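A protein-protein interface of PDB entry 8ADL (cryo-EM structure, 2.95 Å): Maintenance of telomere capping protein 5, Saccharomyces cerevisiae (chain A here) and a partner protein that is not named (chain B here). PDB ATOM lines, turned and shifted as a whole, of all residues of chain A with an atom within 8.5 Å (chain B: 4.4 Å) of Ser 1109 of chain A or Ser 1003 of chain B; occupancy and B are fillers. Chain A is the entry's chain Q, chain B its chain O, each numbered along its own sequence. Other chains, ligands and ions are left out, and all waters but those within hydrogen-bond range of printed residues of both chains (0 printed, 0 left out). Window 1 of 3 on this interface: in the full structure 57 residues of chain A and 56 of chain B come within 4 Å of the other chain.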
ATOM      1  N   THR A1080      13.151   6.731   7.530  1.00  0.00           N
ATOM      2  CA  THR A1080      13.080   5.279   7.474  1.00  0.00           C
ATOM      3  C   THR A1080      11.880   4.857   6.638  1.00  0.00           C
ATOM      4  O   THR A1080      10.749   5.279   6.900  1.00  0.00           O
ATOM      5  CB  THR A1080      12.983   4.692   8.881  1.00  0.00           C
ATOM      6  OG1 THR A1080      11.704   5.010   9.442  1.00  0.00           O
ATOM      7  CG2 THR A1080      14.080   5.258   9.770  1.00  0.00           C
ATOM      8  N   TRP A1082       9.682   1.721   5.035  1.00  0.00           N
ATOM      9  CA  TRP A1082       9.325   0.309   5.002  1.00  0.00           C
ATOM     10  C   TRP A1082       9.367  -0.226   3.576  1.00  0.00           C
ATOM     11  O   TRP A1082       9.040   0.481   2.619  1.00  0.00           O
ATOM     12  CB  TRP A1082       7.931   0.103   5.588  1.00  0.00           C
ATOM     13  CG  TRP A1082       7.810   0.505   7.022  1.00  0.00           C
ATOM     14  CD1 TRP A1082       7.260   1.654   7.506  1.00  0.00           C
ATOM     15  CD2 TRP A1082       8.242  -0.243   8.163  1.00  0.00           C
ATOM     16  NE1 TRP A1082       7.324   1.670   8.877  1.00  0.00           N
ATOM     17  CE2 TRP A1082       7.924   0.516   9.305  1.00  0.00           C
ATOM     18  CE3 TRP A1082       8.869  -1.481   8.330  1.00  0.00           C
ATOM     19  CZ2 TRP A1082       8.208   0.079  10.594  1.00  0.00           C
ATOM     20  CZ3 TRP A1082       9.152  -1.913   9.612  1.00  0.00           C
ATOM     21  CH2 TRP A1082       8.823  -1.134  10.727  1.00  0.00           C
ATOM     22  N   CYS A1098       8.807  -6.465  15.553  1.00  0.00           N
ATOM     23  CA  CYS A1098      10.146  -6.696  16.075  1.00  0.00           C
ATOM     24  C   CYS A1098      10.520  -8.171  15.969  1.00  0.00           C
ATOM     25  O   CYS A1098       9.672  -9.060  16.062  1.00  0.00           O
ATOM     26  CB  CYS A1098      10.225  -6.236  17.533  1.00  0.00           C
ATOM     27  SG  CYS A1098      11.783  -6.578  18.371  1.00  0.00           S
ATOM     28  N   VAL A1105       6.650  -2.438  16.143  1.00  0.00           N
ATOM     29  CA  VAL A1105       7.658  -1.424  16.429  1.00  0.00           C
ATOM     30  C   VAL A1105       7.228  -0.097  15.811  1.00  0.00           C
ATOM     31  O   VAL A1105       6.778  -0.044  14.658  1.00  0.00           O
ATOM     32  CB  VAL A1105       9.060  -1.873  15.964  1.00  0.00           C
ATOM     33  CG1 VAL A1105       9.159  -2.049  14.450  1.00  0.00           C
ATOM     34  CG2 VAL A1105      10.116  -0.897  16.451  1.00  0.00           C
ATOM     35  N   THR A1106       7.258   0.960  16.620  1.00  0.00           N
ATOM     36  CA  THR A1106       6.879   2.288  16.146  1.00  0.00           C
ATOM     37  C   THR A1106       7.805   3.401  16.608  1.00  0.00           C
ATOM     38  O   THR A1106       7.806   4.466  15.980  1.00  0.00           O
ATOM     39  CB  THR A1106       5.447   2.624  16.578  1.00  0.00           C
ATOM     40  OG1 THR A1106       5.108   3.943  16.133  1.00  0.00           O
ATOM     41  CG2 THR A1106       5.307   2.546  18.091  1.00  0.00           C
ATOM     42  N   ARG A1107       8.595   3.209  17.662  1.00  0.00           N
ATOM     43  CA  ARG A1107       9.504   4.227  18.170  1.00  0.00           C
ATOM     44  C   ARG A1107      10.801   3.572  18.615  1.00  0.00           C
ATOM     45  O   ARG A1107      10.782   2.484  19.199  1.00  0.00           O
ATOM     46  CB  ARG A1107       8.873   5.000  19.336  1.00  0.00           C
ATOM     47  CG  ARG A1107       7.801   5.995  18.917  1.00  0.00           C
ATOM     48  CD  ARG A1107       6.642   6.019  19.897  1.00  0.00           C
ATOM     49  NE  ARG A1107       5.639   7.008  19.524  1.00  0.00           N
ATOM     50  CZ  ARG A1107       4.621   7.370  20.293  1.00  0.00           C
ATOM     51  NH1 ARG A1107       4.438   6.840  21.490  1.00  0.00           N
ATOM     52  NH2 ARG A1107       3.766   8.286  19.848  1.00  0.00           N
ATOM     53  N   SER A1108      11.919   4.253  18.338  1.00  0.00           N
ATOM     54  CA  SER A1108      13.258   3.909  18.833  1.00  0.00           C
ATOM     55  C   SER A1108      13.670   2.502  18.390  1.00  0.00           C
ATOM     56  O   SER A1108      13.838   1.582  19.191  1.00  0.00           O
ATOM     57  CB  SER A1108      13.334   4.053  20.358  1.00  0.00           C
ATOM     58  OG  SER A1108      14.677   4.038  20.805  1.00  0.00           O
ATOM     59  N   SER A1109      13.820   2.361  17.079  1.00  0.00           N
ATOM     60  CA  SER A1109      14.146   1.081  16.475  1.00  0.00           C
ATOM     61  C   SER A1109      15.652   0.946  16.260  1.00  0.00           C
ATOM     62  O   SER A1109      16.413   1.908  16.364  1.00  0.00           O
ATOM     63  CB  SER A1109      13.411   0.912  15.145  1.00  0.00           C
ATOM     64  OG  SER A1109      14.120   1.552  14.101  1.00  0.00           O
ATOM     65  N   PHE A1110      16.069  -0.278  15.945  1.00  0.00           N
ATOM     66  CA  PHE A1110      17.425  -0.579  15.504  1.00  0.00           C
ATOM     67  C   PHE A1110      17.354  -1.287  14.161  1.00  0.00           C
ATOM     68  O   PHE A1110      16.646  -2.289  14.021  1.00  0.00           O
ATOM     69  CB  PHE A1110      18.161  -1.447  16.530  1.00  0.00           C
ATOM     70  CG  PHE A1110      19.315  -2.224  15.958  1.00  0.00           C
ATOM     71  CD1 PHE A1110      20.458  -1.577  15.515  1.00  0.00           C
ATOM     72  CD2 PHE A1110      19.262  -3.606  15.879  1.00  0.00           C
ATOM     73  CE1 PHE A1110      21.523  -2.292  14.995  1.00  0.00           C
ATOM     74  CE2 PHE A1110      20.324  -4.327  15.362  1.00  0.00           C
ATOM     75  CZ  PHE A1110      21.454  -3.669  14.920  1.00  0.00           C
ATOM     76  N   ILE A1111      18.088  -0.770  13.178  1.00  0.00           N
ATOM     77  CA  ILE A1111      18.055  -1.288  11.816  1.00  0.00           C
ATOM     78  C   ILE A1111      19.454  -1.743  11.430  1.00  0.00           C
ATOM     79  O   ILE A1111      20.423  -0.987  11.571  1.00  0.00           O
ATOM     80  CB  ILE A1111      17.533  -0.235  10.820  1.00  0.00           C
ATOM     81  CG1 ILE A1111      16.198   0.343  11.293  1.00  0.00           C
ATOM     82  CG2 ILE A1111      17.402  -0.828   9.431  1.00  0.00           C
ATOM     83  CD1 ILE A1111      15.858   1.676  10.670  1.00  0.00           C
ATOM     84  N   CYS A1112      19.555  -2.976  10.945  1.00  0.00           N
ATOM     85  CA  CYS A1112      20.760  -3.496  10.322  1.00  0.00           C
ATOM     86  C   CYS A1112      20.765  -3.188   8.829  1.00  0.00           C
ATOM     87  O   CYS A1112      19.722  -2.962   8.210  1.00  0.00           O
ATOM     88  CB  CYS A1112      20.875  -5.003  10.549  1.00  0.00           C
ATOM     89  SG  CYS A1112      22.347  -5.758   9.826  1.00  0.00           S
ATOM     90  N   HIS A1117      16.067  -5.917   8.956  1.00  0.00           N
ATOM     91  CA  HIS A1117      15.220  -6.368  10.051  1.00  0.00           C
ATOM     92  C   HIS A1117      15.233  -5.354  11.186  1.00  0.00           C
ATOM     93  O   HIS A1117      16.288  -4.820  11.542  1.00  0.00           O
ATOM     94  CB  HIS A1117      15.672  -7.738  10.577  1.00  0.00           C
ATOM     95  CG  HIS A1117      15.475  -8.857   9.603  1.00  0.00           C
ATOM     96  ND1 HIS A1117      16.348  -9.918   9.502  1.00  0.00           N
ATOM     97  CD2 HIS A1117      14.499  -9.084   8.691  1.00  0.00           C
ATOM     98  CE1 HIS A1117      15.922 -10.748   8.568  1.00  0.00           C
ATOM     99  NE2 HIS A1117      14.802 -10.266   8.060  1.00  0.00           N
ATOM    100  N   VAL A1118      14.055  -5.099  11.757  1.00  0.00           N
ATOM    101  CA  VAL A1118      13.907  -4.143  12.847  1.00  0.00           C
ATOM    102  C   VAL A1118      14.131  -4.843  14.180  1.00  0.00           C
ATOM    103  O   VAL A1118      14.008  -6.065  14.300  1.00  0.00           O
ATOM    104  CB  VAL A1118      12.523  -3.465  12.825  1.00  0.00           C
ATOM    105  CG1 VAL A1118      12.389  -2.558  11.632  1.00  0.00           C
ATOM    106  CG2 VAL A1118      11.429  -4.515  12.813  1.00  0.00           C
ATOM    107  N   LEU A1119      14.446  -4.045  15.197  1.00  0.00           N
ATOM    108  CA  LEU A1119      14.399  -4.457  16.592  1.00  0.00           C
ATOM    109  C   LEU A1119      14.020  -3.247  17.433  1.00  0.00           C
ATOM    110  O   LEU A1119      14.310  -2.110  17.061  1.00  0.00           O
ATOM    111  CB  LEU A1119      15.741  -5.016  17.083  1.00  0.00           C
ATOM    112  CG  LEU A1119      16.189  -6.423  16.689  1.00  0.00           C
ATOM    113  CD1 LEU A1119      17.532  -6.744  17.315  1.00  0.00           C
ATOM    114  CD2 LEU A1119      15.146  -7.439  17.111  1.00  0.00           C
ATOM    115  N   HIS A1120      13.367  -3.497  18.566  1.00  0.00           N
ATOM    116  CA  HIS A1120      13.183  -2.435  19.545  1.00  0.00           C
ATOM    117  C   HIS A1120      14.525  -2.077  20.176  1.00  0.00           C
ATOM    118  O   HIS A1120      15.477  -2.862  20.147  1.00  0.00           O
ATOM    119  CB  HIS A1120      12.197  -2.862  20.633  1.00  0.00           C
ATOM    120  CG  HIS A1120      10.769  -2.889  20.187  1.00  0.00           C
ATOM    121  ND1 HIS A1120      10.051  -4.059  20.065  1.00  0.00           N
ATOM    122  CD2 HIS A1120       9.921  -1.889  19.845  1.00  0.00           C
ATOM    123  CE1 HIS A1120       8.824  -3.779  19.662  1.00  0.00           C
ATOM    124  NE2 HIS A1120       8.720  -2.469  19.520  1.00  0.00           N
ATOM    125  N   SER A1121      14.602  -0.870  20.744  1.00  0.00           N
ATOM    126  CA  SER A1121      15.826  -0.455  21.424  1.00  0.00           C
ATOM    127  C   SER A1121      16.092  -1.307  22.659  1.00  0.00           C
ATOM    128  O   SER A1121      17.230  -1.731  22.895  1.00  0.00           O
ATOM    129  CB  SER A1121      15.745   1.022  21.802  1.00  0.00           C
ATOM    130  OG  SER A1121      17.027   1.541  22.105  1.00  0.00           O
ATOM    131  N   SER A1122      15.050  -1.579  23.447  1.00  0.00           N
ATOM    132  CA  SER A1122      15.197  -2.466  24.597  1.00  0.00           C
ATOM    133  C   SER A1122      15.482  -3.896  24.158  1.00  0.00           C
ATOM    134  O   SER A1122      16.314  -4.582  24.761  1.00  0.00           O
ATOM    135  CB  SER A1122      13.942  -2.408  25.468  1.00  0.00           C
ATOM    136  OG  SER A1122      13.754  -1.110  26.003  1.00  0.00           O
ATOM    137  N   ALA A1124      16.959  -4.828  21.347  1.00  0.00           N
ATOM    138  CA  ALA A1124      18.331  -4.883  20.853  1.00  0.00           C
ATOM    139  C   ALA A1124      19.336  -4.835  21.995  1.00  0.00           C
ATOM    140  O   ALA A1124      20.321  -5.581  21.989  1.00  0.00           O
ATOM    141  CB  ALA A1124      18.589  -3.745  19.867  1.00  0.00           C
ATOM    142  N   TRP B1001      25.619   2.155  17.097  1.00  0.00           N
ATOM    143  CA  TRP B1001      24.533   2.247  16.129  1.00  0.00           C
ATOM    144  C   TRP B1001      23.528   3.312  16.540  1.00  0.00           C
ATOM    145  O   TRP B1001      23.327   3.571  17.730  1.00  0.00           O
ATOM    146  CB  TRP B1001      23.813   0.904  15.952  1.00  0.00           C
ATOM    147  CG  TRP B1001      23.474   0.183  17.226  1.00  0.00           C
ATOM    148  CD1 TRP B1001      24.265  -0.701  17.896  1.00  0.00           C
ATOM    149  CD2 TRP B1001      22.238   0.247  17.956  1.00  0.00           C
ATOM    150  NE1 TRP B1001      23.612  -1.178  19.005  1.00  0.00           N
ATOM    151  CE2 TRP B1001      22.366  -0.612  19.066  1.00  0.00           C
ATOM    152  CE3 TRP B1001      21.044   0.956  17.789  1.00  0.00           C
ATOM    153  CZ2 TRP B1001      21.346  -0.787  20.000  1.00  0.00           C
ATOM    154  CZ3 TRP B1001      20.028   0.780  18.720  1.00  0.00           C
ATOM    155  CH2 TRP B1001      20.187  -0.086  19.809  1.00  0.00           C
ATOM    156  N   PHE B1002      22.908   3.940  15.542  1.00  0.00           N
ATOM    157  CA  PHE B1002      21.816   4.864  15.810  1.00  0.00           C
ATOM    158  C   PHE B1002      20.515   4.143  16.128  1.00  0.00           C
ATOM    159  O   PHE B1002      20.157   3.153  15.485  1.00  0.00           O
ATOM    160  CB  PHE B1002      21.573   5.818  14.640  1.00  0.00           C
ATOM    161  CG  PHE B1002      22.592   6.906  14.512  1.00  0.00           C
ATOM    162  CD1 PHE B1002      23.504   7.156  15.524  1.00  0.00           C
ATOM    163  CD2 PHE B1002      22.570   7.750  13.419  1.00  0.00           C
ATOM    164  CE1 PHE B1002      24.418   8.179  15.408  1.00  0.00           C
ATOM    165  CE2 PHE B1002      23.472   8.778  13.302  1.00  0.00           C
ATOM    166  CZ  PHE B1002      24.398   8.990  14.297  1.00  0.00           C
ATOM    167  N   SER B1003      19.811   4.651  17.140  1.00  0.00           N
ATOM    168  CA  SER B1003      18.468   4.193  17.475  1.00  0.00           C
ATOM    169  C   SER B1003      17.481   5.145  16.805  1.00  0.00           C
ATOM    170  O   SER B1003      16.980   6.096  17.404  1.00  0.00           O
ATOM    171  CB  SER B1003      18.270   4.134  18.984  1.00  0.00           C
ATOM    172  OG  SER B1003      16.892   4.063  19.306  1.00  0.00           O
ATOM    173  N   PHE B1004      17.195   4.872  15.536  1.00  0.00           N
ATOM    174  CA  PHE B1004      16.312   5.722  14.749  1.00  0.00           C
ATOM    175  C   PHE B1004      14.859   5.471  15.129  1.00  0.00           C
ATOM    176  O   PHE B1004      14.379   4.335  15.048  1.00  0.00           O
ATOM    177  CB  PHE B1004      16.510   5.467  13.257  1.00  0.00           C
ATOM    178  CG  PHE B1004      17.507   6.376  12.611  1.00  0.00           C
ATOM    179  CD1 PHE B1004      17.173   7.686  12.310  1.00  0.00           C
ATOM    180  CD2 PHE B1004      18.773   5.920  12.289  1.00  0.00           C
ATOM    181  CE1 PHE B1004      18.088   8.528  11.707  1.00  0.00           C
ATOM    182  CE2 PHE B1004      19.690   6.754  11.684  1.00  0.00           C
ATOM    183  CZ  PHE B1004      19.348   8.061  11.395  1.00  0.00           C
ATOM    184  N   CYS B1005      14.161   6.526  15.536  1.00  0.00           N
ATOM    185  CA  CYS B1005      12.721   6.432  15.719  1.00  0.00           C
ATOM    186  C   CYS B1005      12.037   6.380  14.361  1.00  0.00           C
ATOM    187  O   CYS B1005      12.458   7.045  13.410  1.00  0.00           O
ATOM    188  CB  CYS B1005      12.200   7.616  16.530  1.00  0.00           C
ATOM    189  SG  CYS B1005      10.403   7.619  16.740  1.00  0.00           S
ATOM    190  N   LEU B1006      10.980   5.583  14.269  1.00  0.00           N
ATOM    191  CA  LEU B1006      10.237   5.428  13.027  1.00  0.00           C
ATOM    192  C   LEU B1006       9.057   6.384  12.913  1.00  0.00           C
ATOM    193  O   LEU B1006       8.299   6.297  11.942  1.00  0.00           O
ATOM    194  CB  LEU B1006       9.748   3.982  12.899  1.00  0.00           C
ATOM    195  CG  LEU B1006      10.836   2.941  13.166  1.00  0.00           C
ATOM    196  CD1 LEU B1006      10.271   1.537  13.135  1.00  0.00           C
ATOM    197  CD2 LEU B1006      11.958   3.084  12.156  1.00  0.00           C
ATOM    198  N   HIS B1010      14.430  10.825  13.853  1.00  0.00           N
ATOM    199  CA  HIS B1010      15.592  11.449  14.471  1.00  0.00           C
ATOM    200  C   HIS B1010      16.431  10.391  15.172  1.00  0.00           C
ATOM    201  O   HIS B1010      15.903   9.587  15.945  1.00  0.00           O
ATOM    202  CB  HIS B1010      15.163  12.538  15.455  1.00  0.00           C
ATOM    203  CG  HIS B1010      14.368  13.638  14.824  1.00  0.00           C
ATOM    204  ND1 HIS B1010      13.234  14.166  15.401  1.00  0.00           N
ATOM    205  CD2 HIS B1010      14.547  14.310  13.663  1.00  0.00           C
ATOM    206  CE1 HIS B1010      12.747  15.115  14.621  1.00  0.00           C
ATOM    207  NE2 HIS B1010      13.525  15.222  13.561  1.00  0.00           N
ATOM    208  N   GLY B1011      17.733  10.401  14.909  1.00  0.00           N
ATOM    209  CA  GLY B1011      18.631   9.343  15.352  1.00  0.00           C
ATOM    210  C   GLY B1011      19.645   9.819  16.376  1.00  0.00           C
ATOM    211  O   GLY B1011      20.212  10.908  16.250  1.00  0.00           O
ATOM    212  N   MET B1012      19.868   8.981  17.386  1.00  0.00           N
ATOM    213  CA  MET B1012      20.906   9.157  18.389  1.00  0.00           C
ATOM    214  C   MET B1012      21.642   7.837  18.545  1.00  0.00           C
ATOM    215  O   MET B1012      21.091   6.773  18.258  1.00  0.00           O
ATOM    216  CB  MET B1012      20.330   9.549  19.754  1.00  0.00           C
ATOM    217  CG  MET B1012      19.226  10.575  19.735  1.00  0.00           C
ATOM    218  SD  MET B1012      18.249  10.405  21.235  1.00  0.00           S
ATOM    219  CE  MET B1012      19.407  11.032  22.442  1.00  0.00           C
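OG of Ser 1108 of chain A lies within hydrogen-bond range of OG of Ser 1003 of chain B (2.7 Å). N of Ser 1109 of chain A is in hydrogen-bond range of O of Phe 1004 of chain B (2.9 Å).
Printed residues of chain B within 4 Å of Thr 1080 of chain A: Leu 1006 (3.3 Å). His 1120 of chain A touches none of the printed residues of chain B. Printed residues of chain B within 4 Å of Ser 1121 of chain A: Ser 1003. Printed residues of chain A within 4 Å of Ser 1003 of chain B: Ser 1108, Ser 1109 and Ser 1121. Printed residues of chain A within 4 Å of Phe 1004 of chain B: Ser 1108 (3.9 Å) and Ser 1109 (2.9 Å). Of the printed residues of chain A, Cys 1005 of chain B touches Arg 1107 and Ser 1108. Of the printed residues of chain A, Leu 1006 of chain B touches Thr 1080, Trp 1082, Val 1105, Thr 1106 and Ser 1109.
Of the 18 printed residues of chain A, 10 touch a printed residue of chain B. Hydrophobic or aromatic side chains of chain B that line the printed part of chain A: Trp 1001 and Leu 1006.
N of Ser 1121 of chain A sits at hydrogen-bond distance from O of Ser 1108 of chain A (3.0 Å). N of Ser 1003 of chain B lies within hydrogen-bond range of O of Met 1012 of chain B, at 2.7 Å. N of Phe 1110 of chain A sits at hydrogen-bond distance from O of Leu 1119 of chain A, 2.8 Å away.
Leu 1006 of chain B touches Thr 1080 of chain A. Trp 1082 of chain A touches Leu 1006 of chain B. Val 1105 of chain A touches Leu 1006 of chain B. Thr 1106 of chain A touches Leu 1006 of chain B. CG of Arg 1107 of chain A touches SG of Cys 1005 of chain B, 3.8 Å away. Ser 1109 of chain A touches Ser 1003 of chain B. OG of Ser 1109 of chain A touches CD2 of Leu 1006 of chain B (3.3 Å). Phe 1110 of chain A touches Trp 1001 of chain B (CD1 to CE3, 3.5 Å). OG of Ser 1121 of chain A touches OG of Ser 1003 of chain B, 3.8 Å away. Ala 1124 of chain A touches Trp 1001 of chain B (CB to CH2, 3.99 Å).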
